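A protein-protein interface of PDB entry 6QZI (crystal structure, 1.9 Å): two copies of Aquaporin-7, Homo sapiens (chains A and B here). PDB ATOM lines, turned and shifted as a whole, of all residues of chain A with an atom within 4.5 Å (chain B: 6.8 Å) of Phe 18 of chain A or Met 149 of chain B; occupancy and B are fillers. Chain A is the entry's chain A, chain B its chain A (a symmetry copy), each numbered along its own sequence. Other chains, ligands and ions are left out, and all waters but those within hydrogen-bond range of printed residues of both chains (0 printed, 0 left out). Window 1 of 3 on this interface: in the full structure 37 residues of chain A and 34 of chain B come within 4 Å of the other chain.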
ATOM      1  N   TYR A  13     -14.171 -23.885  16.704  1.00  0.00           N
ATOM      2  CA  TYR A  13     -13.377 -25.024  17.159  1.00  0.00           C
ATOM      3  C   TYR A  13     -12.443 -24.620  18.294  1.00  0.00           C
ATOM      4  O   TYR A  13     -12.403 -25.271  19.344  1.00  0.00           O
ATOM      5  CB  TYR A  13     -12.573 -25.614  15.996  1.00  0.00           C
ATOM      6  CG  TYR A  13     -11.655 -26.738  16.429  1.00  0.00           C
ATOM      7  CD1 TYR A  13     -12.126 -28.041  16.535  1.00  0.00           C
ATOM      8  CD2 TYR A  13     -10.321 -26.496  16.741  1.00  0.00           C
ATOM      9  CE1 TYR A  13     -11.296 -29.072  16.940  1.00  0.00           C
ATOM     10  CE2 TYR A  13      -9.483 -27.521  17.146  1.00  0.00           C
ATOM     11  CZ  TYR A  13      -9.976 -28.806  17.246  1.00  0.00           C
ATOM     12  OH  TYR A  13      -9.146 -29.829  17.648  1.00  0.00           O
ATOM     13  N   VAL A  14     -11.675 -23.549  18.089  1.00  0.00           N
ATOM     14  CA  VAL A  14     -10.727 -23.096  19.103  1.00  0.00           C
ATOM     15  C   VAL A  14     -11.458 -22.748  20.394  1.00  0.00           C
ATOM     16  O   VAL A  14     -11.086 -23.203  21.483  1.00  0.00           O
ATOM     17  CB  VAL A  14      -9.916 -21.899  18.573  1.00  0.00           C
ATOM     18  CG1 VAL A  14      -9.175 -21.205  19.709  1.00  0.00           C
ATOM     19  CG2 VAL A  14      -8.947 -22.351  17.488  1.00  0.00           C
ATOM     20  N   MET A  15     -12.512 -21.935  20.289  1.00  0.00           N
ATOM     21  CA  MET A  15     -13.263 -21.533  21.475  1.00  0.00           C
ATOM     22  C   MET A  15     -13.791 -22.741  22.235  1.00  0.00           C
ATOM     23  O   MET A  15     -13.730 -22.785  23.470  1.00  0.00           O
ATOM     24  CB  MET A  15     -14.418 -20.613  21.074  1.00  0.00           C
ATOM     25  CG  MET A  15     -15.277 -20.146  22.237  1.00  0.00           C
ATOM     26  SD  MET A  15     -16.669 -21.232  22.610  1.00  0.00           S
ATOM     27  CE  MET A  15     -17.751 -20.901  21.211  1.00  0.00           C
ATOM     28  N   MET A  16     -14.311 -23.735  21.515  1.00  0.00           N
ATOM     29  CA  MET A  16     -14.960 -24.864  22.171  1.00  0.00           C
ATOM     30  C   MET A  16     -13.959 -25.846  22.769  1.00  0.00           C
ATOM     31  O   MET A  16     -14.275 -26.514  23.759  1.00  0.00           O
ATOM     32  CB  MET A  16     -15.887 -25.573  21.183  1.00  0.00           C
ATOM     33  CG  MET A  16     -17.145 -24.779  20.858  1.00  0.00           C
ATOM     34  SD  MET A  16     -18.250 -24.650  22.277  1.00  0.00           S
ATOM     35  CE  MET A  16     -18.681 -26.375  22.513  1.00  0.00           C
ATOM     36  N   VAL A  17     -12.759 -25.959  22.196  1.00  0.00           N
ATOM     37  CA  VAL A  17     -11.725 -26.780  22.823  1.00  0.00           C
ATOM     38  C   VAL A  17     -11.358 -26.207  24.187  1.00  0.00           C
ATOM     39  O   VAL A  17     -11.271 -26.930  25.186  1.00  0.00           O
ATOM     40  CB  VAL A  17     -10.491 -26.890  21.909  1.00  0.00           C
ATOM     41  CG1 VAL A  17      -9.315 -27.469  22.683  1.00  0.00           C
ATOM     42  CG2 VAL A  17     -10.801 -27.749  20.684  1.00  0.00           C
ATOM     43  N   PHE A  18     -11.136 -24.892  24.246  1.00  0.00           N
ATOM     44  CA  PHE A  18     -10.858 -24.247  25.526  1.00  0.00           C
ATOM     45  C   PHE A  18     -12.056 -24.352  26.462  1.00  0.00           C
ATOM     46  O   PHE A  18     -11.899 -24.620  27.658  1.00  0.00           O
ATOM     47  CB  PHE A  18     -10.479 -22.782  25.303  1.00  0.00           C
ATOM     48  CG  PHE A  18      -9.096 -22.587  24.735  1.00  0.00           C
ATOM     49  CD1 PHE A  18      -7.975 -22.992  25.443  1.00  0.00           C
ATOM     50  CD2 PHE A  18      -8.920 -21.994  23.495  1.00  0.00           C
ATOM     51  CE1 PHE A  18      -6.701 -22.813  24.923  1.00  0.00           C
ATOM     52  CE2 PHE A  18      -7.650 -21.810  22.969  1.00  0.00           C
ATOM     53  CZ  PHE A  18      -6.539 -22.221  23.685  1.00  0.00           C
ATOM     54  N   GLY A  19     -13.260 -24.144  25.937  1.00  0.00           N
ATOM     55  CA  GLY A  19     -14.454 -24.222  26.755  1.00  0.00           C
ATOM     56  C   GLY A  19     -14.705 -25.600  27.333  1.00  0.00           C
ATOM     57  O   GLY A  19     -14.791 -25.767  28.554  1.00  0.00           O
ATOM     58  N   LEU A  20     -14.818 -26.601  26.459  1.00  0.00           N
ATOM     59  CA  LEU A  20     -15.127 -27.950  26.919  1.00  0.00           C
ATOM     60  C   LEU A  20     -13.988 -28.538  27.743  1.00  0.00           C
ATOM     61  O   LEU A  20     -14.234 -29.316  28.671  1.00  0.00           O
ATOM     62  CB  LEU A  20     -15.443 -28.848  25.724  1.00  0.00           C
ATOM     63  CG  LEU A  20     -16.688 -28.457  24.922  1.00  0.00           C
ATOM     64  CD1 LEU A  20     -16.998 -29.499  23.849  1.00  0.00           C
ATOM     65  CD2 LEU A  20     -17.885 -28.262  25.846  1.00  0.00           C
ATOM     66  N   GLY A  21     -12.745 -28.185  27.422  1.00  0.00           N
ATOM     67  CA  GLY A  21     -11.631 -28.656  28.225  1.00  0.00           C
ATOM     68  C   GLY A  21     -11.710 -28.193  29.668  1.00  0.00           C
ATOM     69  O   GLY A  21     -11.420 -28.960  30.589  1.00  0.00           O
ATOM     70  N   SER A  22     -12.109 -26.934  29.888  1.00  0.00           N
ATOM     71  CA  SER A  22     -12.189 -26.435  31.259  1.00  0.00           C
ATOM     72  C   SER A  22     -13.310 -27.116  32.027  1.00  0.00           C
ATOM     73  O   SER A  22     -13.190 -27.326  33.239  1.00  0.00           O
ATOM     74  CB  SER A  22     -12.393 -24.914  31.288  1.00  0.00           C
ATOM     75  OG  SER A  22     -13.544 -24.510  30.565  1.00  0.00           O
ATOM     76  N   GLY A  41     -12.142 -20.500  30.958  1.00  0.00           N
ATOM     77  CA  GLY A  41     -11.856 -21.266  29.754  1.00  0.00           C
ATOM     78  C   GLY A  41     -12.758 -20.887  28.595  1.00  0.00           C
ATOM     79  O   GLY A  41     -12.291 -20.665  27.474  1.00  0.00           O
ATOM     80  N   GLY A  45     -11.381 -18.456  25.847  1.00  0.00           N
ATOM     81  CA  GLY A  45     -11.501 -19.207  24.609  1.00  0.00           C
ATOM     82  C   GLY A  45     -12.210 -18.408  23.532  1.00  0.00           C
ATOM     83  O   GLY A  45     -11.857 -18.484  22.352  1.00  0.00           O
ATOM     84  N   MET A  48      -9.684 -15.950  21.986  1.00  0.00           N
ATOM     85  CA  MET A  48      -8.841 -16.526  20.944  1.00  0.00           C
ATOM     86  C   MET A  48      -9.616 -16.698  19.640  1.00  0.00           C
ATOM     87  O   MET A  48      -9.082 -16.434  18.560  1.00  0.00           O
ATOM     88  CB  MET A  48      -8.262 -17.859  21.419  1.00  0.00           C
ATOM     89  CG  MET A  48      -7.452 -17.731  22.709  1.00  0.00           C
ATOM     90  SD  MET A  48      -6.146 -16.495  22.568  1.00  0.00           S
ATOM     91  CE  MET A  48      -6.104 -15.855  24.243  1.00  0.00           C
ATOM     92  N   ALA B 144       1.202 -32.941  21.645  1.00  0.00           N
ATOM     93  CA  ALA B 144       1.169 -32.473  20.264  1.00  0.00           C
ATOM     94  C   ALA B 144      -0.009 -31.533  20.031  1.00  0.00           C
ATOM     95  O   ALA B 144       0.157 -30.434  19.492  1.00  0.00           O
ATOM     96  CB  ALA B 144       1.109 -33.663  19.303  1.00  0.00           C
ATOM     97  N   TRP B 145      -1.211 -31.944  20.442  1.00  0.00           N
ATOM     98  CA  TRP B 145      -2.393 -31.133  20.166  1.00  0.00           C
ATOM     99  C   TRP B 145      -2.347 -29.809  20.916  1.00  0.00           C
ATOM    100  O   TRP B 145      -2.702 -28.762  20.363  1.00  0.00           O
ATOM    101  CB  TRP B 145      -3.662 -31.903  20.522  1.00  0.00           C
ATOM    102  CG  TRP B 145      -4.796 -31.592  19.604  1.00  0.00           C
ATOM    103  CD1 TRP B 145      -5.647 -30.528  19.681  1.00  0.00           C
ATOM    104  CD2 TRP B 145      -5.193 -32.344  18.452  1.00  0.00           C
ATOM    105  NE1 TRP B 145      -6.556 -30.576  18.652  1.00  0.00           N
ATOM    106  CE2 TRP B 145      -6.299 -31.681  17.884  1.00  0.00           C
ATOM    107  CE3 TRP B 145      -4.724 -33.515  17.851  1.00  0.00           C
ATOM    108  CZ2 TRP B 145      -6.942 -32.152  16.742  1.00  0.00           C
ATOM    109  CZ3 TRP B 145      -5.365 -33.980  16.716  1.00  0.00           C
ATOM    110  CH2 TRP B 145      -6.462 -33.299  16.173  1.00  0.00           C
ATOM    111  N   LEU B 146      -1.905 -29.836  22.173  1.00  0.00           N
ATOM    112  CA  LEU B 146      -1.860 -28.612  22.965  1.00  0.00           C
ATOM    113  C   LEU B 146      -0.841 -27.630  22.403  1.00  0.00           C
ATOM    114  O   LEU B 146      -1.088 -26.418  22.377  1.00  0.00           O
ATOM    115  CB  LEU B 146      -1.540 -28.942  24.423  1.00  0.00           C
ATOM    116  CG  LEU B 146      -2.681 -29.305  25.377  1.00  0.00           C
ATOM    117  CD1 LEU B 146      -3.676 -30.287  24.760  1.00  0.00           C
ATOM    118  CD2 LEU B 146      -2.110 -29.877  26.669  1.00  0.00           C
ATOM    119  N   THR B 147       0.315 -28.130  21.957  1.00  0.00           N
ATOM    120  CA  THR B 147       1.292 -27.248  21.325  1.00  0.00           C
ATOM    121  C   THR B 147       0.786 -26.747  19.979  1.00  0.00           C
ATOM    122  O   THR B 147       1.120 -25.629  19.569  1.00  0.00           O
ATOM    123  CB  THR B 147       2.634 -27.967  21.163  1.00  0.00           C
ATOM    124  OG1 THR B 147       2.978 -28.623  22.388  1.00  0.00           O
ATOM    125  CG2 THR B 147       3.731 -26.978  20.817  1.00  0.00           C
ATOM    126  N   GLY B 148      -0.014 -27.555  19.281  1.00  0.00           N
ATOM    127  CA  GLY B 148      -0.678 -27.066  18.086  1.00  0.00           C
ATOM    128  C   GLY B 148      -1.631 -25.925  18.383  1.00  0.00           C
ATOM    129  O   GLY B 148      -1.660 -24.924  17.662  1.00  0.00           O
ATOM    130  N   MET B 149      -2.425 -26.059  19.449  1.00  0.00           N
ATOM    131  CA  MET B 149      -3.298 -24.963  19.863  1.00  0.00           C
ATOM    132  C   MET B 149      -2.491 -23.715  20.186  1.00  0.00           C
ATOM    133  O   MET B 149      -2.890 -22.597  19.835  1.00  0.00           O
ATOM    134  CB  MET B 149      -4.134 -25.382  21.074  1.00  0.00           C
ATOM    135  CG  MET B 149      -5.124 -26.515  20.800  1.00  0.00           C
ATOM    136  SD  MET B 149      -6.549 -25.965  19.836  1.00  0.00           S
ATOM    137  CE  MET B 149      -7.237 -24.717  20.924  1.00  0.00           C
ATOM    138  N   LEU B 150      -1.352 -23.888  20.861  1.00  0.00           N
ATOM    139  CA  LEU B 150      -0.496 -22.753  21.187  1.00  0.00           C
ATOM    140  C   LEU B 150      -0.025 -22.038  19.925  1.00  0.00           C
ATOM    141  O   LEU B 150      -0.157 -20.815  19.803  1.00  0.00           O
ATOM    142  CB  LEU B 150       0.703 -23.223  22.014  1.00  0.00           C
ATOM    143  CG  LEU B 150       1.778 -22.171  22.302  1.00  0.00           C
ATOM    144  CD1 LEU B 150       1.293 -21.193  23.363  1.00  0.00           C
ATOM    145  CD2 LEU B 150       3.084 -22.831  22.736  1.00  0.00           C
ATOM    146  N   GLN B 151       0.517 -22.791  18.966  1.00  0.00           N
ATOM    147  CA  GLN B 151       1.105 -22.159  17.790  1.00  0.00           C
ATOM    148  C   GLN B 151       0.043 -21.481  16.929  1.00  0.00           C
ATOM    149  O   GLN B 151       0.268 -20.383  16.404  1.00  0.00           O
ATOM    150  CB  GLN B 151       1.881 -23.187  16.972  1.00  0.00           C
ATOM    151  CG  GLN B 151       2.748 -22.567  15.889  1.00  0.00           C
ATOM    152  CD  GLN B 151       3.767 -21.596  16.456  1.00  0.00           C
ATOM    153  OE1 GLN B 151       4.774 -22.004  17.036  1.00  0.00           O
ATOM    154  NE2 GLN B 151       3.507 -20.301  16.296  1.00  0.00           N
ATOM    155  N   LEU B 152      -1.121 -22.115  16.774  1.00  0.00           N
ATOM    156  CA  LEU B 152      -2.179 -21.522  15.964  1.00  0.00           C
ATOM    157  C   LEU B 152      -2.662 -20.209  16.568  1.00  0.00           C
ATOM    158  O   LEU B 152      -2.825 -19.209  15.860  1.00  0.00           O
ATOM    159  CB  LEU B 152      -3.342 -22.504  15.810  1.00  0.00           C
ATOM    160  CG  LEU B 152      -4.513 -22.020  14.950  1.00  0.00           C
ATOM    161  CD1 LEU B 152      -5.013 -23.135  14.043  1.00  0.00           C
ATOM    162  CD2 LEU B 152      -5.646 -21.489  15.819  1.00  0.00           C
ATOM    163  N   CYS B 153      -2.900 -20.196  17.884  1.00  0.00           N
ATOM    164  CA  CYS B 153      -3.349 -18.969  18.527  1.00  0.00           C
ATOM    165  C   CYS B 153      -2.240 -17.927  18.607  1.00  0.00           C
ATOM    166  O   CYS B 153      -2.521 -16.729  18.516  1.00  0.00           O
ATOM    167  CB  CYS B 153      -3.907 -19.276  19.916  1.00  0.00           C
ATOM    168  SG  CYS B 153      -5.386 -20.315  19.873  1.00  0.00           S
ATOM    169  N   LEU B 154      -0.986 -18.350  18.783  1.00  0.00           N
ATOM    170  CA  LEU B 154       0.127 -17.405  18.723  1.00  0.00           C
ATOM    171  C   LEU B 154       0.125 -16.663  17.395  1.00  0.00           C
ATOM    172  O   LEU B 154       0.264 -15.435  17.352  1.00  0.00           O
ATOM    173  CB  LEU B 154       1.455 -18.137  18.918  1.00  0.00           C
ATOM    174  CG  LEU B 154       1.919 -18.508  20.326  1.00  0.00           C
ATOM    175  CD1 LEU B 154       3.338 -19.059  20.263  1.00  0.00           C
ATOM    176  CD2 LEU B 154       1.837 -17.321  21.274  1.00  0.00           C
ATOM    177  N   ILE B 176      -2.445 -14.681  28.357  1.00  0.00           N
ATOM    178  CA  ILE B 176      -3.764 -15.252  28.616  1.00  0.00           C
ATOM    179  C   ILE B 176      -3.927 -16.576  27.882  1.00  0.00           C
ATOM    180  O   ILE B 176      -4.528 -17.523  28.403  1.00  0.00           O
ATOM    181  CB  ILE B 176      -4.858 -14.241  28.228  1.00  0.00           C
ATOM    182  CG1 ILE B 176      -4.887 -13.105  29.248  1.00  0.00           C
ATOM    183  CG2 ILE B 176      -6.218 -14.923  28.129  1.00  0.00           C
ATOM    184  CD1 ILE B 176      -5.610 -11.878  28.777  1.00  0.00           C
ATOM    185  N   LEU B 177      -3.402 -16.662  26.657  1.00  0.00           N
ATOM    186  CA  LEU B 177      -3.419 -17.923  25.924  1.00  0.00           C
ATOM    187  C   LEU B 177      -2.757 -19.036  26.731  1.00  0.00           C
ATOM    188  O   LEU B 177      -3.306 -20.136  26.864  1.00  0.00           O
ATOM    189  CB  LEU B 177      -2.719 -17.749  24.577  1.00  0.00           C
ATOM    190  CG  LEU B 177      -2.366 -19.024  23.809  1.00  0.00           C
ATOM    191  CD1 LEU B 177      -3.626 -19.803  23.446  1.00  0.00           C
ATOM    192  CD2 LEU B 177      -1.551 -18.683  22.567  1.00  0.00           C
ATOM    193  N   ILE B 180      -4.969 -20.200  29.729  1.00  0.00           N
ATOM    194  CA  ILE B 180      -6.105 -21.086  29.503  1.00  0.00           C
ATOM    195  C   ILE B 180      -5.707 -22.411  28.871  1.00  0.00           C
ATOM    196  O   ILE B 180      -6.482 -23.369  28.944  1.00  0.00           O
ATOM    197  CB  ILE B 180      -7.197 -20.424  28.645  1.00  0.00           C
ATOM    198  CG1 ILE B 180      -6.646 -20.005  27.281  1.00  0.00           C
ATOM    199  CG2 ILE B 180      -7.818 -19.251  29.395  1.00  0.00           C
ATOM    200  CD1 ILE B 180      -7.722 -19.508  26.328  1.00  0.00           C
ATOM    201  N   ILE B 181      -4.537 -22.508  28.237  1.00  0.00           N
ATOM    202  CA  ILE B 181      -4.045 -23.838  27.892  1.00  0.00           C
ATOM    203  C   ILE B 181      -3.905 -24.672  29.158  1.00  0.00           C
ATOM    204  O   ILE B 181      -4.278 -25.851  29.192  1.00  0.00           O
ATOM    205  CB  ILE B 181      -2.721 -23.750  27.108  1.00  0.00           C
ATOM    206  CG1 ILE B 181      -2.982 -23.216  25.697  1.00  0.00           C
ATOM    207  CG2 ILE B 181      -2.050 -25.121  27.030  1.00  0.00           C
ATOM    208  CD1 ILE B 181      -1.724 -22.935  24.902  1.00  0.00           C
ATOM    209  N   GLY B 182      -3.421 -24.053  30.236  1.00  0.00           N
ATOM    210  CA  GLY B 182      -3.387 -24.739  31.517  1.00  0.00           C
ATOM    211  C   GLY B 182      -4.769 -24.975  32.098  1.00  0.00           C
ATOM    212  O   GLY B 182      -5.072 -26.074  32.569  1.00  0.00           O
ATOM    213  N   VAL B 183      -5.627 -23.953  32.066  1.00  0.00           N
ATOM    214  CA  VAL B 183      -6.964 -24.086  32.645  1.00  0.00           C
ATOM    215  C   VAL B 183      -7.744 -25.196  31.950  1.00  0.00           C
ATOM    216  O   VAL B 183      -8.396 -26.018  32.601  1.00  0.00           O
ATOM    217  CB  VAL B 183      -7.721 -22.744  32.559  1.00  0.00           C
ATOM    218  CG1 VAL B 183      -9.188 -22.939  32.923  1.00  0.00           C
ATOM    219  CG2 VAL B 183      -7.075 -21.686  33.455  1.00  0.00           C
ATOM    220  N   SER B 184      -7.690 -25.232  30.618  1.00  0.00           N
ATOM    221  CA  SER B 184      -8.569 -26.086  29.826  1.00  0.00           C
ATOM    222  C   SER B 184      -7.970 -27.434  29.456  1.00  0.00           C
ATOM    223  O   SER B 184      -8.724 -28.381  29.224  1.00  0.00           O
ATOM    224  CB  SER B 184      -8.975 -25.372  28.530  1.00  0.00           C
ATOM    225  OG  SER B 184      -9.504 -24.082  28.782  1.00  0.00           O
ATOM    226  N   LEU B 185      -6.645 -27.555  29.372  1.00  0.00           N
ATOM    227  CA  LEU B 185      -6.044 -28.733  28.758  1.00  0.00           C
ATOM    228  C   LEU B 185      -4.887 -29.331  29.553  1.00  0.00           C
ATOM    229  O   LEU B 185      -4.259 -30.284  29.078  1.00  0.00           O
ATOM    230  CB  LEU B 185      -5.560 -28.389  27.341  1.00  0.00           C
ATOM    231  CG  LEU B 185      -6.615 -27.838  26.377  1.00  0.00           C
ATOM    232  CD1 LEU B 185      -5.973 -27.201  25.152  1.00  0.00           C
ATOM    233  CD2 LEU B 185      -7.572 -28.957  25.977  1.00  0.00           C
ATOM    234  N   GLY B 232       3.583 -30.825  17.098  1.00  0.00           N
ATOM    235  CA  GLY B 232       2.343 -30.091  17.295  1.00  0.00           C
ATOM    236  C   GLY B 232       2.443 -28.645  16.853  1.00  0.00           C
ATOM    237  O   GLY B 232       1.562 -28.131  16.160  1.00  0.00           O
ATOM    238  N   ALA B 233       3.525 -27.969  17.246  1.00  0.00           N
ATOM    239  CA  ALA B 233       3.710 -26.577  16.849  1.00  0.00           C
ATOM    240  C   ALA B 233       3.738 -26.436  15.333  1.00  0.00           C
ATOM    241  O   ALA B 233       3.104 -25.534  14.773  1.00  0.00           O
ATOM    242  CB  ALA B 233       4.993 -26.018  17.463  1.00  0.00           C
ATOM    243  N   GLY B 236       0.139 -27.044  14.046  1.00  0.00           N
ATOM    244  CA  GLY B 236      -0.725 -25.917  14.362  1.00  0.00           C
ATOM    245  C   GLY B 236      -0.429 -24.703  13.505  1.00  0.00           C
ATOM    246  O   GLY B 236      -1.345 -24.007  13.059  1.00  0.00           O
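The side-chain hydroxyl of Ser 184 of chain B sits at hydrogen-bond distance from the backbone carbonyl oxygen of Phe 18 of chain A (2.7 Å).
The backbone carbonyl oxygen of Ser 184 of chain B sits close to the backbone carbonyl oxygen of Gly 21 of chain A, at 3.1 Å.
The side-chain hydroxyl (OH) of Tyr 13 of chain A is in hydrogen-bond range of the indole nitrogen (NE1) of Trp 145 of chain B.
The side-chain sulfur (SG) of Cys 153 of chain B is in hydrogen-bond range of the backbone carbonyl oxygen (O) of Met 149 of chain B, at 3.4 Å.
The backbone carbonyl oxygen (O) of Phe 18 of chain A lies within hydrogen-bond range of the side-chain hydroxyl (OG) of Ser 22 of chain A, at 3.3 Å.
The backbone carbonyl oxygen of Ile 180 of chain B sits at hydrogen-bond distance from the side-chain hydroxyl of Ser 184 of chain B (3.1 Å).
The backbone carbonyl oxygen of Gly 19 of chain A lies within hydrogen-bond range of the side-chain hydroxyl of Ser 22 of chain A (2.7 Å).
Of chain B, only Met 149, Leu 177, Ile 180, Ile 181 and Ser 184 come within 4 Å of Phe 18 of chain A.
Printed residues of chain A within 4 Å of Trp 145 of chain B: Tyr 13.
Of chain A, only Val 17 and Phe 18 come within 4 Å of Met 149 of chain B.
Gly 182 of chain B touches none of the printed residues of chain A.
Printed residues of chain A within 4 Å of Ser 184 of chain B: Phe 18, Gly 21, Ser 22 and Gly 41.
The nearest residue of chain A that does not touch Met 149 of chain B is Val 14 of chain A (4.2 Å).
The nearest printed residue of chain B that does not touch Ser 22 of chain A is Val 183 of chain B (4.04 Å).
Of the 22 printed residues of chain B, 9 touch a printed residue of chain A.
Hydrophobic or aromatic side chains of chain B that line the printed part of chain A: Trp 145, Met 149, Leu 152, Ile 176, Leu 177, Ile 180 and Ile 181.
Of the 13 printed residues of chain A, 9 touch a printed residue of chain B.
Hydrophobic or aromatic side chains of chain A within 4 Å of the printed part of chain B: Tyr 13, Val 14, Val 17, Phe 18 and Met 48.
Along chain A the printed residues that touch a printed residue of chain B span positions 13 to 48.
Among the printed residues, 15 pairs touch across the chains.
Among the printed residues, no Asp or Glu carboxylate lies within 4 Å of a Lys or Arg side-chain nitrogen of the other chain.
No position is printed for both chains.
Among the printed residues, pairs that only touch across the chains: Val 14 of chain A with Leu 152 of chain B (3.8 Å), Val 14 of chain A with Cys 153 of chain B (3.9 Å), Val 17 of chain A with Met 149 of chain B (3.9 Å), Phe 18 of chain A with Met 149 of chain B (3.6 Å), Phe 18 of chain A with Leu 177 of chain B (3.8 Å), Phe 18 of chain A with Ile 180 of chain B (3.6 Å), Phe 18 of chain A with Ile 181 of chain B (3.8 Å), Ser 22 of chain A with Ser 184 of chain B (3.6 Å), Gly 41 of chain A with Ser 184 of chain B (3.8 Å), Gly 45 of chain A with Ile 180 of chain B (3.8 Å), Met 48 of chain A with Ile 176 of chain B (3.998 Å) and Met 48 of chain A with Leu 177 of chain B (3.7 Å).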
